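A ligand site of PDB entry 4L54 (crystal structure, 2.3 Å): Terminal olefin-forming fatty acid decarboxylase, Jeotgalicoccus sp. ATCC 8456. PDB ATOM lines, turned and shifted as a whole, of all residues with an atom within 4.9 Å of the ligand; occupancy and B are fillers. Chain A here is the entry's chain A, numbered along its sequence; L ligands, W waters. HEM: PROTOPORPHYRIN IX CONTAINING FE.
A ring nitrogen (ND1) of His 363 is in hydrogen-bond range of an oxygen (O2D) of the ligand, at 2.8 Å. The side-chain hydroxyl of Tyr 59 is in hydrogen-bond range of an oxygen (O1A) of the ligand, at 2.4 Å. An oxygen (O2A) of the ligand lies within salt-bridge range of the guanidinium group (NH2) of Arg 66. O1D of the ligand is in salt-bridge range of NZ of Lys 96 (2.6 Å). An oxygen (O1D) of the ligand sits at hydrogen-bond distance from a ring nitrogen (NE2) of His 92, 2.8 Å away. The side-chain sulfur of Cys 365 is bound to an iron atom (FE) of the ligand.
The backbone NH (N) of Cys 365 lies close to the backbone carbonyl oxygen (O) of Gln 354, at 3.2 Å. The backbone NH of Gly 367 lies close to the side-chain sulfur of Cys 365. The backbone carbonyl oxygen (O) of Gly 367 lies within hydrogen-bond range of the side-chain hydroxyl (OG1) of Thr 371. The backbone carbonyl oxygen (O) of Arg 364 sits at hydrogen-bond distance from the side-chain amino group (NZ) of Lys 96, at 2.6 Å. A ring nitrogen (NE2) of His 92 sits at hydrogen-bond distance from a ring nitrogen (ND1) of His 363 (3.4 Å). The side-chain amino group (NZ) of Lys 96 sits at hydrogen-bond distance from the backbone carbonyl oxygen (O) of Asn 362. The side-chain hydroxyl (OG1) of Thr 371 sits at hydrogen-bond distance from the side-chain amide oxygen (OE1) of Gln 354 (3.3 Å). The backbone carbonyl oxygen (O) of Tyr 59 is in hydrogen-bond range of the side-chain amide nitrogen (ND2) of Asn 362.
NB of the ligand sits close to OE1 of Gln 354, at 3.3 Å. CG2 of Ile 84 touches CAD of the ligand, 3.8 Å away. His 85 touches the ligand. Phe 99 touches the ligand (CE2 to CMD, 3.4 Å). O of Asn 242 touches CMD of the ligand, at 3.7 Å. O of Thr 243 touches CBC of the ligand, 3.2 Å away. Pro 246 touches the ligand (CB to C1C, 3.2 Å). Leu 247 touches the ligand (CA to CMC, 3.4 Å). Ala 249 touches the ligand. Ile 250 touches the ligand (N to CBB, 3.7 Å). Phe 253 touches the ligand. Phe 291 touches the ligand (CE1 to CBB, 3.6 Å). Val 292 touches the ligand (CG2 to CMA, 3.8 Å). CD1 of Leu 295 touches O1A of the ligand, 3.8 Å away. CA of Gly 355 touches CBA of the ligand, 3.9 Å away. Asn 362 touches the ligand (O to O1D, 3.7 Å). O of Arg 364 touches CBD of the ligand (3.7 Å). N of Ala 366 touches C1D of the ligand, at 3.7 Å. Gly 367 touches the ligand (CA to C3C, 3.5 Å). CD1 of Ile 370 touches CBC of the ligand (3.9 Å). Thr 371 touches the ligand. Hydrophobic or aromatic side chains within 4 Å of the ligand: Tyr 59, Ile 84, His 85, His 92, Phe 99, Pro 246, Leu 247, Ala 249, Phe 253, Phe 291, Val 292, Leu 295, His 363, Ala 366 and Ile 370.
Water W2 bridges the backbone carbonyl oxygen of Asn 242 (3.2 Å) and a ring nitrogen (NE2) of His 85 (3.3 Å).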
ATOM      1  N   TYR A  59     -20.077  -2.338  -7.830  1.00  0.00           N
ATOM      2  CA  TYR A  59     -21.319  -3.059  -7.540  1.00  0.00           C
ATOM      3  C   TYR A  59     -21.638  -4.140  -8.541  1.00  0.00           C
ATOM      4  O   TYR A  59     -22.748  -4.604  -8.599  1.00  0.00           O
ATOM      5  CB  TYR A  59     -22.463  -2.053  -7.435  1.00  0.00           C
ATOM      6  CG  TYR A  59     -22.419  -1.246  -6.162  1.00  0.00           C
ATOM      7  CD1 TYR A  59     -22.660  -1.849  -4.934  1.00  0.00           C
ATOM      8  CD2 TYR A  59     -22.124   0.103  -6.172  1.00  0.00           C
ATOM      9  CE1 TYR A  59     -22.610  -1.154  -3.762  1.00  0.00           C
ATOM     10  CE2 TYR A  59     -22.078   0.837  -4.992  1.00  0.00           C
ATOM     11  CZ  TYR A  59     -22.315   0.185  -3.774  1.00  0.00           C
ATOM     12  OH  TYR A  59     -22.279   0.887  -2.594  1.00  0.00           O
ATOM     13  N   ARG A  66     -17.481  -8.202  -1.136  1.00  0.00           N
ATOM     14  CA  ARG A  66     -17.561  -7.282   0.033  1.00  0.00           C
ATOM     15  C   ARG A  66     -17.261  -7.971   1.357  1.00  0.00           C
ATOM     16  O   ARG A  66     -16.647  -7.402   2.232  1.00  0.00           O
ATOM     17  CB  ARG A  66     -18.955  -6.635   0.137  1.00  0.00           C
ATOM     18  CG  ARG A  66     -19.389  -5.882  -1.110  1.00  0.00           C
ATOM     19  CD  ARG A  66     -18.478  -4.709  -1.443  1.00  0.00           C
ATOM     20  NE  ARG A  66     -18.543  -3.679  -0.406  1.00  0.00           N
ATOM     21  CZ  ARG A  66     -19.526  -2.798  -0.273  1.00  0.00           C
ATOM     22  NH1 ARG A  66     -20.523  -2.756  -1.139  1.00  0.00           N
ATOM     23  NH2 ARG A  66     -19.473  -1.926   0.735  1.00  0.00           N
ATOM     24  N   ILE A  84     -25.800  -7.743   8.525  1.00  0.00           N
ATOM     25  CA  ILE A  84     -26.015  -7.847   7.054  1.00  0.00           C
ATOM     26  C   ILE A  84     -24.850  -7.281   6.243  1.00  0.00           C
ATOM     27  O   ILE A  84     -24.449  -7.878   5.232  1.00  0.00           O
ATOM     28  CB  ILE A  84     -27.339  -7.219   6.635  1.00  0.00           C
ATOM     29  CG1 ILE A  84     -27.640  -7.568   5.173  1.00  0.00           C
ATOM     30  CG2 ILE A  84     -27.344  -5.734   6.834  1.00  0.00           C
ATOM     31  CD1 ILE A  84     -29.054  -7.624   4.854  1.00  0.00           C
ATOM     32  N   HIS A  85     -24.260  -6.191   6.722  1.00  0.00           N
ATOM     33  CA  HIS A  85     -23.113  -5.598   6.019  1.00  0.00           C
ATOM     34  C   HIS A  85     -21.977  -6.604   5.760  1.00  0.00           C
ATOM     35  O   HIS A  85     -21.186  -6.384   4.875  1.00  0.00           O
ATOM     36  CB  HIS A  85     -22.541  -4.442   6.813  1.00  0.00           C
ATOM     37  CG  HIS A  85     -23.545  -3.422   7.209  1.00  0.00           C
ATOM     38  ND1 HIS A  85     -24.512  -3.663   8.168  1.00  0.00           N
ATOM     39  CD2 HIS A  85     -23.728  -2.141   6.785  1.00  0.00           C
ATOM     40  CE1 HIS A  85     -25.254  -2.577   8.304  1.00  0.00           C
ATOM     41  NE2 HIS A  85     -24.801  -1.640   7.480  1.00  0.00           N
ATOM     42  N   HIS A  92     -27.018 -13.045   1.788  1.00  0.00           N
ATOM     43  CA  HIS A  92     -27.236 -11.632   1.753  1.00  0.00           C
ATOM     44  C   HIS A  92     -28.548 -11.205   1.073  1.00  0.00           C
ATOM     45  O   HIS A  92     -29.158 -10.249   1.497  1.00  0.00           O
ATOM     46  CB  HIS A  92     -26.057 -10.888   1.076  1.00  0.00           C
ATOM     47  CG  HIS A  92     -26.316  -9.438   0.947  1.00  0.00           C
ATOM     48  ND1 HIS A  92     -26.732  -8.863  -0.227  1.00  0.00           N
ATOM     49  CD2 HIS A  92     -26.358  -8.469   1.891  1.00  0.00           C
ATOM     50  CE1 HIS A  92     -26.962  -7.584  -0.016  1.00  0.00           C
ATOM     51  NE2 HIS A  92     -26.731  -7.315   1.261  1.00  0.00           N
ATOM     52  N   LYS A  96     -31.387  -9.205   2.998  1.00  0.00           N
ATOM     53  CA  LYS A  96     -31.633  -7.900   2.481  1.00  0.00           C
ATOM     54  C   LYS A  96     -33.093  -7.770   2.135  1.00  0.00           C
ATOM     55  O   LYS A  96     -33.679  -6.691   2.368  1.00  0.00           O
ATOM     56  CB  LYS A  96     -30.786  -7.558   1.232  1.00  0.00           C
ATOM     57  CG  LYS A  96     -31.023  -6.113   0.686  1.00  0.00           C
ATOM     58  CD  LYS A  96     -30.653  -5.030   1.749  1.00  0.00           C
ATOM     59  CE  LYS A  96     -30.312  -3.675   1.137  1.00  0.00           C
ATOM     60  NZ  LYS A  96     -29.033  -3.608   0.411  1.00  0.00           N
ATOM     61  N   PHE A  99     -34.982  -6.599   5.146  1.00  0.00           N
ATOM     62  CA  PHE A  99     -34.869  -5.187   5.402  1.00  0.00           C
ATOM     63  C   PHE A  99     -35.756  -4.370   4.499  1.00  0.00           C
ATOM     64  O   PHE A  99     -36.435  -3.512   4.972  1.00  0.00           O
ATOM     65  CB  PHE A  99     -33.426  -4.687   5.272  1.00  0.00           C
ATOM     66  CG  PHE A  99     -32.587  -4.908   6.496  1.00  0.00           C
ATOM     67  CD1 PHE A  99     -31.977  -6.128   6.705  1.00  0.00           C
ATOM     68  CD2 PHE A  99     -32.420  -3.892   7.449  1.00  0.00           C
ATOM     69  CE1 PHE A  99     -31.206  -6.327   7.791  1.00  0.00           C
ATOM     70  CE2 PHE A  99     -31.597  -4.097   8.540  1.00  0.00           C
ATOM     71  CZ  PHE A  99     -30.997  -5.311   8.715  1.00  0.00           C
ATOM     72  N   MET A 103     -39.881  -1.371   3.931  1.00  0.00           N
ATOM     73  CA  MET A 103     -40.008  -0.106   3.262  1.00  0.00           C
ATOM     74  C   MET A 103     -41.189  -0.068   2.287  1.00  0.00           C
ATOM     75  O   MET A 103     -41.048   0.266   1.079  1.00  0.00           O
ATOM     76  CB  MET A 103     -38.712   0.284   2.565  1.00  0.00           C
ATOM     77  CG  MET A 103     -37.441   0.073   3.324  1.00  0.00           C
ATOM     78  SD  MET A 103     -37.423   1.000   4.845  1.00  0.00           S
ATOM     79  CE  MET A 103     -36.029   0.250   5.782  1.00  0.00           C
ATOM     80  N   TRP A 149     -40.753   3.556  15.275  1.00  0.00           N
ATOM     81  CA  TRP A 149     -40.887   3.060  13.946  1.00  0.00           C
ATOM     82  C   TRP A 149     -40.559   1.559  13.912  1.00  0.00           C
ATOM     83  O   TRP A 149     -41.300   0.794  13.337  1.00  0.00           O
ATOM     84  CB  TRP A 149     -40.003   3.863  12.961  1.00  0.00           C
ATOM     85  CG  TRP A 149     -40.159   3.347  11.576  1.00  0.00           C
ATOM     86  CD1 TRP A 149     -41.213   3.530  10.745  1.00  0.00           C
ATOM     87  CD2 TRP A 149     -39.255   2.491  10.889  1.00  0.00           C
ATOM     88  NE1 TRP A 149     -41.020   2.856   9.576  1.00  0.00           N
ATOM     89  CE2 TRP A 149     -39.822   2.220   9.633  1.00  0.00           C
ATOM     90  CE3 TRP A 149     -38.032   1.938  11.202  1.00  0.00           C
ATOM     91  CZ2 TRP A 149     -39.205   1.399   8.711  1.00  0.00           C
ATOM     92  CZ3 TRP A 149     -37.408   1.136  10.287  1.00  0.00           C
ATOM     93  CH2 TRP A 149     -37.998   0.856   9.065  1.00  0.00           C
ATOM     94  N   ASN A 242     -29.644  -2.402  13.203  1.00  0.00           N
ATOM     95  CA  ASN A 242     -29.269  -1.906  11.899  1.00  0.00           C
ATOM     96  C   ASN A 242     -30.475  -1.323  11.153  1.00  0.00           C
ATOM     97  O   ASN A 242     -30.361  -0.772  10.074  1.00  0.00           O
ATOM     98  CB  ASN A 242     -28.564  -3.000  11.096  1.00  0.00           C
ATOM     99  CG  ASN A 242     -27.136  -3.199  11.566  1.00  0.00           C
ATOM    100  OD1 ASN A 242     -26.531  -2.267  12.068  1.00  0.00           O
ATOM    101  ND2 ASN A 242     -26.616  -4.424  11.460  1.00  0.00           N
ATOM    102  N   THR A 243     -31.609  -1.416  11.772  1.00  0.00           N
ATOM    103  CA  THR A 243     -32.824  -0.926  11.174  1.00  0.00           C
ATOM    104  C   THR A 243     -33.178   0.483  11.699  1.00  0.00           C
ATOM    105  O   THR A 243     -34.048   1.159  11.137  1.00  0.00           O
ATOM    106  CB  THR A 243     -33.918  -1.929  11.505  1.00  0.00           C
ATOM    107  OG1 THR A 243     -34.436  -2.514  10.301  1.00  0.00           O
ATOM    108  CG2 THR A 243     -34.934  -1.394  12.456  1.00  0.00           C
ATOM    109  N   PHE A 244     -32.503   0.936  12.764  1.00  0.00           N
ATOM    110  CA  PHE A 244     -32.819   2.237  13.276  1.00  0.00           C
ATOM    111  C   PHE A 244     -31.672   3.042  13.929  1.00  0.00           C
ATOM    112  O   PHE A 244     -31.800   4.250  14.127  1.00  0.00           O
ATOM    113  CB  PHE A 244     -34.058   2.122  14.157  1.00  0.00           C
ATOM    114  CG  PHE A 244     -33.774   1.553  15.493  1.00  0.00           C
ATOM    115  CD1 PHE A 244     -33.854   0.180  15.704  1.00  0.00           C
ATOM    116  CD2 PHE A 244     -33.386   2.383  16.545  1.00  0.00           C
ATOM    117  CE1 PHE A 244     -33.590  -0.335  16.915  1.00  0.00           C
ATOM    118  CE2 PHE A 244     -33.119   1.861  17.745  1.00  0.00           C
ATOM    119  CZ  PHE A 244     -33.218   0.498  17.952  1.00  0.00           C
ATOM    120  N   PRO A 246     -29.066   3.706  12.206  1.00  0.00           N
ATOM    121  CA  PRO A 246     -28.758   4.682  11.133  1.00  0.00           C
ATOM    122  C   PRO A 246     -29.842   5.744  10.947  1.00  0.00           C
ATOM    123  O   PRO A 246     -29.539   6.840  10.477  1.00  0.00           O
ATOM    124  CB  PRO A 246     -28.644   3.821   9.893  1.00  0.00           C
ATOM    125  CG  PRO A 246     -28.494   2.427  10.354  1.00  0.00           C
ATOM    126  CD  PRO A 246     -29.195   2.335  11.693  1.00  0.00           C
ATOM    127  N   LEU A 247     -31.077   5.432  11.293  1.00  0.00           N
ATOM    128  CA  LEU A 247     -32.135   6.440  11.277  1.00  0.00           C
ATOM    129  C   LEU A 247     -31.771   7.548  12.267  1.00  0.00           C
ATOM    130  O   LEU A 247     -31.883   8.726  11.974  1.00  0.00           O
ATOM    131  CB  LEU A 247     -33.465   5.766  11.601  1.00  0.00           C
ATOM    132  CG  LEU A 247     -34.781   6.521  11.661  1.00  0.00           C
ATOM    133  CD1 LEU A 247     -35.954   5.503  11.830  1.00  0.00           C
ATOM    134  CD2 LEU A 247     -34.793   7.543  12.759  1.00  0.00           C
ATOM    135  N   ALA A 249     -28.830   8.320  13.135  1.00  0.00           N
ATOM    136  CA  ALA A 249     -27.635   8.931  12.563  1.00  0.00           C
ATOM    137  C   ALA A 249     -27.981  10.034  11.593  1.00  0.00           C
ATOM    138  O   ALA A 249     -27.122  10.829  11.184  1.00  0.00           O
ATOM    139  CB  ALA A 249     -26.793   7.846  11.821  1.00  0.00           C
ATOM    140  N   ILE A 250     -29.250  10.090  11.189  1.00  0.00           N
ATOM    141  CA  ILE A 250     -29.729  11.216  10.351  1.00  0.00           C
ATOM    142  C   ILE A 250     -29.572  12.554  11.083  1.00  0.00           C
ATOM    143  O   ILE A 250     -29.689  13.638  10.451  1.00  0.00           O
ATOM    144  CB  ILE A 250     -31.198  11.013   9.923  1.00  0.00           C
ATOM    145  CG1 ILE A 250     -31.342   9.742   9.124  1.00  0.00           C
ATOM    146  CG2 ILE A 250     -31.737  12.130   9.105  1.00  0.00           C
ATOM    147  CD1 ILE A 250     -32.790   9.289   8.970  1.00  0.00           C
ATOM    148  N   PHE A 253     -27.272  14.803   9.444  1.00  0.00           N
ATOM    149  CA  PHE A 253     -27.756  15.566   8.279  1.00  0.00           C
ATOM    150  C   PHE A 253     -28.670  16.709   8.715  1.00  0.00           C
ATOM    151  O   PHE A 253     -28.808  17.654   7.999  1.00  0.00           O
ATOM    152  CB  PHE A 253     -28.488  14.662   7.239  1.00  0.00           C
ATOM    153  CG  PHE A 253     -27.566  13.796   6.414  1.00  0.00           C
ATOM    154  CD1 PHE A 253     -26.378  14.282   5.897  1.00  0.00           C
ATOM    155  CD2 PHE A 253     -27.910  12.464   6.117  1.00  0.00           C
ATOM    156  CE1 PHE A 253     -25.539  13.489   5.125  1.00  0.00           C
ATOM    157  CE2 PHE A 253     -27.068  11.664   5.334  1.00  0.00           C
ATOM    158  CZ  PHE A 253     -25.885  12.178   4.832  1.00  0.00           C
ATOM    159  N   PHE A 291     -20.028  12.499   4.987  1.00  0.00           N
ATOM    160  CA  PHE A 291     -20.373  11.535   5.984  1.00  0.00           C
ATOM    161  C   PHE A 291     -19.560  10.269   5.656  1.00  0.00           C
ATOM    162  O   PHE A 291     -18.586   9.989   6.327  1.00  0.00           O
ATOM    163  CB  PHE A 291     -21.880  11.256   5.959  1.00  0.00           C
ATOM    164  CG  PHE A 291     -22.397  10.577   7.191  1.00  0.00           C
ATOM    165  CD1 PHE A 291     -23.546  11.028   7.803  1.00  0.00           C
ATOM    166  CD2 PHE A 291     -21.770   9.495   7.733  1.00  0.00           C
ATOM    167  CE1 PHE A 291     -24.029  10.393   8.938  1.00  0.00           C
ATOM    168  CE2 PHE A 291     -22.254   8.863   8.900  1.00  0.00           C
ATOM    169  CZ  PHE A 291     -23.364   9.301   9.491  1.00  0.00           C
ATOM    170  N   VAL A 292     -20.000   9.515   4.658  1.00  0.00           N
ATOM    171  CA  VAL A 292     -19.286   8.303   4.276  1.00  0.00           C
ATOM    172  C   VAL A 292     -18.138   8.632   3.315  1.00  0.00           C
ATOM    173  O   VAL A 292     -18.375   9.045   2.209  1.00  0.00           O
ATOM    174  CB  VAL A 292     -20.192   7.225   3.611  1.00  0.00           C
ATOM    175  CG1 VAL A 292     -19.388   5.955   3.398  1.00  0.00           C
ATOM    176  CG2 VAL A 292     -21.389   6.900   4.533  1.00  0.00           C
ATOM    177  N   LEU A 295     -15.910   3.021   0.609  1.00  0.00           N
ATOM    178  CA  LEU A 295     -16.380   1.677   0.960  1.00  0.00           C
ATOM    179  C   LEU A 295     -15.403   0.629   0.492  1.00  0.00           C
ATOM    180  O   LEU A 295     -14.953   0.724  -0.619  1.00  0.00           O
ATOM    181  CB  LEU A 295     -17.758   1.400   0.340  1.00  0.00           C
ATOM    182  CG  LEU A 295     -18.799   2.434   0.749  1.00  0.00           C
ATOM    183  CD1 LEU A 295     -20.000   2.377  -0.169  1.00  0.00           C
ATOM    184  CD2 LEU A 295     -19.153   2.185   2.250  1.00  0.00           C
ATOM    185  N   PRO A 353     -24.200   8.777  -1.804  1.00  0.00           N
ATOM    186  CA  PRO A 353     -23.600   9.008  -0.492  1.00  0.00           C
ATOM    187  C   PRO A 353     -24.038   7.970   0.530  1.00  0.00           C
ATOM    188  O   PRO A 353     -23.475   7.914   1.630  1.00  0.00           O
ATOM    189  CB  PRO A 353     -24.160  10.386  -0.103  1.00  0.00           C
ATOM    190  CG  PRO A 353     -25.589  10.330  -0.678  1.00  0.00           C
ATOM    191  CD  PRO A 353     -25.362   9.646  -2.032  1.00  0.00           C
ATOM    192  N   GLN A 354     -25.070   7.195   0.176  1.00  0.00           N
ATOM    193  CA  GLN A 354     -25.502   6.024   0.951  1.00  0.00           C
ATOM    194  C   GLN A 354     -25.357   4.755   0.114  1.00  0.00           C
ATOM    195  O   GLN A 354     -26.157   3.830   0.186  1.00  0.00           O
ATOM    196  CB  GLN A 354     -26.937   6.196   1.451  1.00  0.00           C
ATOM    197  CG  GLN A 354     -27.117   7.506   2.176  1.00  0.00           C
ATOM    198  CD  GLN A 354     -28.479   7.698   2.858  1.00  0.00           C
ATOM    199  OE1 GLN A 354     -29.001   6.810   3.517  1.00  0.00           O
ATOM    200  NE2 GLN A 354     -29.026   8.860   2.712  1.00  0.00           N
ATOM    201  N   GLY A 355     -24.329   4.706  -0.707  1.00  0.00           N
ATOM    202  CA  GLY A 355     -24.118   3.542  -1.583  1.00  0.00           C
ATOM    203  C   GLY A 355     -24.787   3.675  -2.952  1.00  0.00           C
ATOM    204  O   GLY A 355     -25.547   4.564  -3.207  1.00  0.00           O
ATOM    205  N   ASN A 362     -27.405  -5.615  -4.218  1.00  0.00           N
ATOM    206  CA  ASN A 362     -26.194  -4.998  -3.674  1.00  0.00           C
ATOM    207  C   ASN A 362     -26.357  -4.611  -2.194  1.00  0.00           C
ATOM    208  O   ASN A 362     -27.454  -4.729  -1.589  1.00  0.00           O
ATOM    209  CB  ASN A 362     -25.865  -3.762  -4.460  1.00  0.00           C
ATOM    210  CG  ASN A 362     -25.443  -4.064  -5.894  1.00  0.00           C
ATOM    211  OD1 ASN A 362     -26.015  -3.519  -6.837  1.00  0.00           O
ATOM    212  ND2 ASN A 362     -24.408  -4.883  -6.058  1.00  0.00           N
ATOM    213  N   HIS A 363     -25.263  -4.143  -1.618  1.00  0.00           N
ATOM    214  CA  HIS A 363     -25.230  -3.708  -0.242  1.00  0.00           C
ATOM    215  C   HIS A 363     -25.707  -2.254  -0.088  1.00  0.00           C
ATOM    216  O   HIS A 363     -25.539  -1.648   0.964  1.00  0.00           O
ATOM    217  CB  HIS A 363     -23.798  -3.830   0.303  1.00  0.00           C
ATOM    218  CG  HIS A 363     -23.450  -5.218   0.716  1.00  0.00           C
ATOM    219  ND1 HIS A 363     -23.846  -5.748   1.929  1.00  0.00           N
ATOM    220  CD2 HIS A 363     -22.754  -6.184   0.081  1.00  0.00           C
ATOM    221  CE1 HIS A 363     -23.378  -6.979   2.031  1.00  0.00           C
ATOM    222  NE2 HIS A 363     -22.704  -7.267   0.929  1.00  0.00           N
ATOM    223  N   ARG A 364     -26.280  -1.695  -1.148  1.00  0.00           N
ATOM    224  CA  ARG A 364     -26.799  -0.350  -1.078  1.00  0.00           C
ATOM    225  C   ARG A 364     -27.706  -0.144   0.172  1.00  0.00           C
ATOM    226  O   ARG A 364     -28.486  -1.036   0.542  1.00  0.00           O
ATOM    227  CB  ARG A 364     -27.613  -0.083  -2.315  1.00  0.00           C
ATOM    228  CG  ARG A 364     -28.032   1.366  -2.413  1.00  0.00           C
ATOM    229  CD  ARG A 364     -28.846   1.675  -3.650  1.00  0.00           C
ATOM    230  NE  ARG A 364     -28.883   3.097  -3.804  1.00  0.00           N
ATOM    231  CZ  ARG A 364     -28.657   3.771  -4.934  1.00  0.00           C
ATOM    232  NH1 ARG A 364     -28.429   3.158  -6.086  1.00  0.00           N
ATOM    233  NH2 ARG A 364     -28.694   5.084  -4.907  1.00  0.00           N
ATOM    234  N   CYS A 365     -27.653   1.048   0.724  1.00  0.00           N
ATOM    235  CA  CYS A 365     -28.379   1.431   1.938  1.00  0.00           C
ATOM    236  C   CYS A 365     -29.875   1.136   1.794  1.00  0.00           C
ATOM    237  O   CYS A 365     -30.514   1.494   0.836  1.00  0.00           O
ATOM    238  CB  CYS A 365     -28.156   2.918   2.272  1.00  0.00           C
ATOM    239  SG  CYS A 365     -28.954   3.486   3.799  1.00  0.00           S
ATOM    240  N   ALA A 366     -30.427   0.436   2.769  1.00  0.00           N
ATOM    241  CA  ALA A 366     -31.834   0.083   2.794  1.00  0.00           C
ATOM    242  C   ALA A 366     -32.722   1.291   3.125  1.00  0.00           C
ATOM    243  O   ALA A 366     -33.906   1.271   2.874  1.00  0.00           O
ATOM    244  CB  ALA A 366     -32.042  -0.978   3.828  1.00  0.00           C
ATOM    245  N   GLY A 367     -32.144   2.339   3.699  1.00  0.00           N
ATOM    246  CA  GLY A 367     -32.898   3.407   4.315  1.00  0.00           C
ATOM    247  C   GLY A 367     -32.754   4.759   3.687  1.00  0.00           C
ATOM    248  O   GLY A 367     -32.975   5.775   4.329  1.00  0.00           O
ATOM    249  N   ILE A 370     -36.181   6.543   3.732  1.00  0.00           N
ATOM    250  CA  ILE A 370     -36.403   7.118   5.073  1.00  0.00           C
ATOM    251  C   ILE A 370     -35.519   8.318   5.291  1.00  0.00           C
ATOM    252  O   ILE A 370     -35.929   9.300   5.868  1.00  0.00           O
ATOM    253  CB  ILE A 370     -36.141   6.095   6.217  1.00  0.00           C
ATOM    254  CG1 ILE A 370     -37.315   5.107   6.239  1.00  0.00           C
ATOM    255  CG2 ILE A 370     -35.920   6.866   7.533  1.00  0.00           C
ATOM    256  CD1 ILE A 370     -37.107   3.816   6.920  1.00  0.00           C
ATOM    257  N   THR A 371     -34.295   8.267   4.811  1.00  0.00           N
ATOM    258  CA  THR A 371     -33.417   9.373   5.081  1.00  0.00           C
ATOM    259  C   THR A 371     -33.975  10.653   4.458  1.00  0.00           C
ATOM    260  O   THR A 371     -34.088  11.663   5.125  1.00  0.00           O
ATOM    261  CB  THR A 371     -31.959   9.031   4.669  1.00  0.00           C
ATOM    262  OG1 THR A 371     -31.551   7.818   5.352  1.00  0.00           O
ATOM    263  CG2 THR A 371     -31.016  10.173   4.992  1.00  0.00           C
HETATM  264  CHA HEM L   1     -26.028   0.450   4.247  1.00  0.00           C
HETATM  265  CHB HEM L   1     -25.112   5.119   4.550  1.00  0.00           C
HETATM  266  CHC HEM L   1     -29.191   5.763   6.963  1.00  0.00           C
HETATM  267  CHD HEM L   1     -30.066   1.064   6.722  1.00  0.00           C
HETATM  268  C1A HEM L   1     -25.451   1.646   4.105  1.00  0.00           C
HETATM  269  C2A HEM L   1     -24.233   1.884   3.365  1.00  0.00           C
HETATM  270  C3A HEM L   1     -23.977   3.172   3.436  1.00  0.00           C
HETATM  271  C4A HEM L   1     -25.055   3.792   4.201  1.00  0.00           C
HETATM  272  CMA HEM L   1     -22.746   3.842   2.792  1.00  0.00           C
HETATM  273  CAA HEM L   1     -23.333   0.821   2.638  1.00  0.00           C
HETATM  274  CBA HEM L   1     -23.539   0.740   1.110  1.00  0.00           C
HETATM  275  CGA HEM L   1     -22.630  -0.347   0.599  1.00  0.00           C
HETATM  276  O1A HEM L   1     -22.457  -0.520  -0.621  1.00  0.00           O
HETATM  277  O2A HEM L   1     -22.014  -1.073   1.395  1.00  0.00           O
HETATM  278  C1B HEM L   1     -26.066   5.679   5.356  1.00  0.00           C
HETATM  279  C2B HEM L   1     -26.073   7.049   5.863  1.00  0.00           C
HETATM  280  C3B HEM L   1     -27.200   7.201   6.543  1.00  0.00           C
HETATM  281  C4B HEM L   1     -27.940   5.976   6.457  1.00  0.00           C
HETATM  282  CMB HEM L   1     -24.970   8.121   5.651  1.00  0.00           C
HETATM  283  CAB HEM L   1     -27.673   8.494   7.226  1.00  0.00           C
HETATM  284  CBB HEM L   1     -27.185   8.826   8.403  1.00  0.00           C
HETATM  285  C1C HEM L   1     -29.848   4.555   7.030  1.00  0.00           C
HETATM  286  C2C HEM L   1     -31.198   4.317   7.516  1.00  0.00           C
HETATM  287  C3C HEM L   1     -31.410   3.017   7.470  1.00  0.00           C
HETATM  288  C4C HEM L   1     -30.235   2.393   6.912  1.00  0.00           C
HETATM  289  CMC HEM L   1     -32.180   5.360   8.057  1.00  0.00           C
HETATM  290  CAC HEM L   1     -32.651   2.241   7.878  1.00  0.00           C
HETATM  291  CBC HEM L   1     -33.687   2.814   8.440  1.00  0.00           C
HETATM  292  C1D HEM L   1     -28.978   0.500   6.136  1.00  0.00           C
HETATM  293  C2D HEM L   1     -28.788  -0.925   6.072  1.00  0.00           C
HETATM  294  C3D HEM L   1     -27.564  -1.135   5.271  1.00  0.00           C
HETATM  295  C4D HEM L   1     -27.126   0.199   4.950  1.00  0.00           C
HETATM  296  CMD HEM L   1     -29.662  -2.033   6.651  1.00  0.00           C
HETATM  297  CAD HEM L   1     -26.894  -2.482   4.928  1.00  0.00           C
HETATM  298  CBD HEM L   1     -27.405  -2.887   3.552  1.00  0.00           C
HETATM  299  CGD HEM L   1     -26.805  -4.166   3.048  1.00  0.00           C
HETATM  300  O1D HEM L   1     -27.427  -4.726   2.075  1.00  0.00           O
HETATM  301  O2D HEM L   1     -25.725  -4.571   3.575  1.00  0.00           O
HETATM  302  NA  HEM L   1     -25.958   2.819   4.562  1.00  0.00           N
HETATM  303  NB  HEM L   1     -27.240   5.072   5.719  1.00  0.00           N
HETATM  304  NC  HEM L   1     -29.318   3.345   6.659  1.00  0.00           N
HETATM  305  ND  HEM L   1     -27.991   1.151   5.434  1.00  0.00           N
HETATM  306 FE   HEM L   1     -27.645   3.079   5.526  1.00  0.00          FE
HETATM  307  O   HOH W   1     -26.144   2.273   7.770  1.00  0.00           O
HETATM  308  O   HOH W   2     -27.329  -0.289   9.155  1.00  0.00           O
HETATM  309  O   HOH W   3     -22.922  -2.443   3.477  1.00  0.00           O
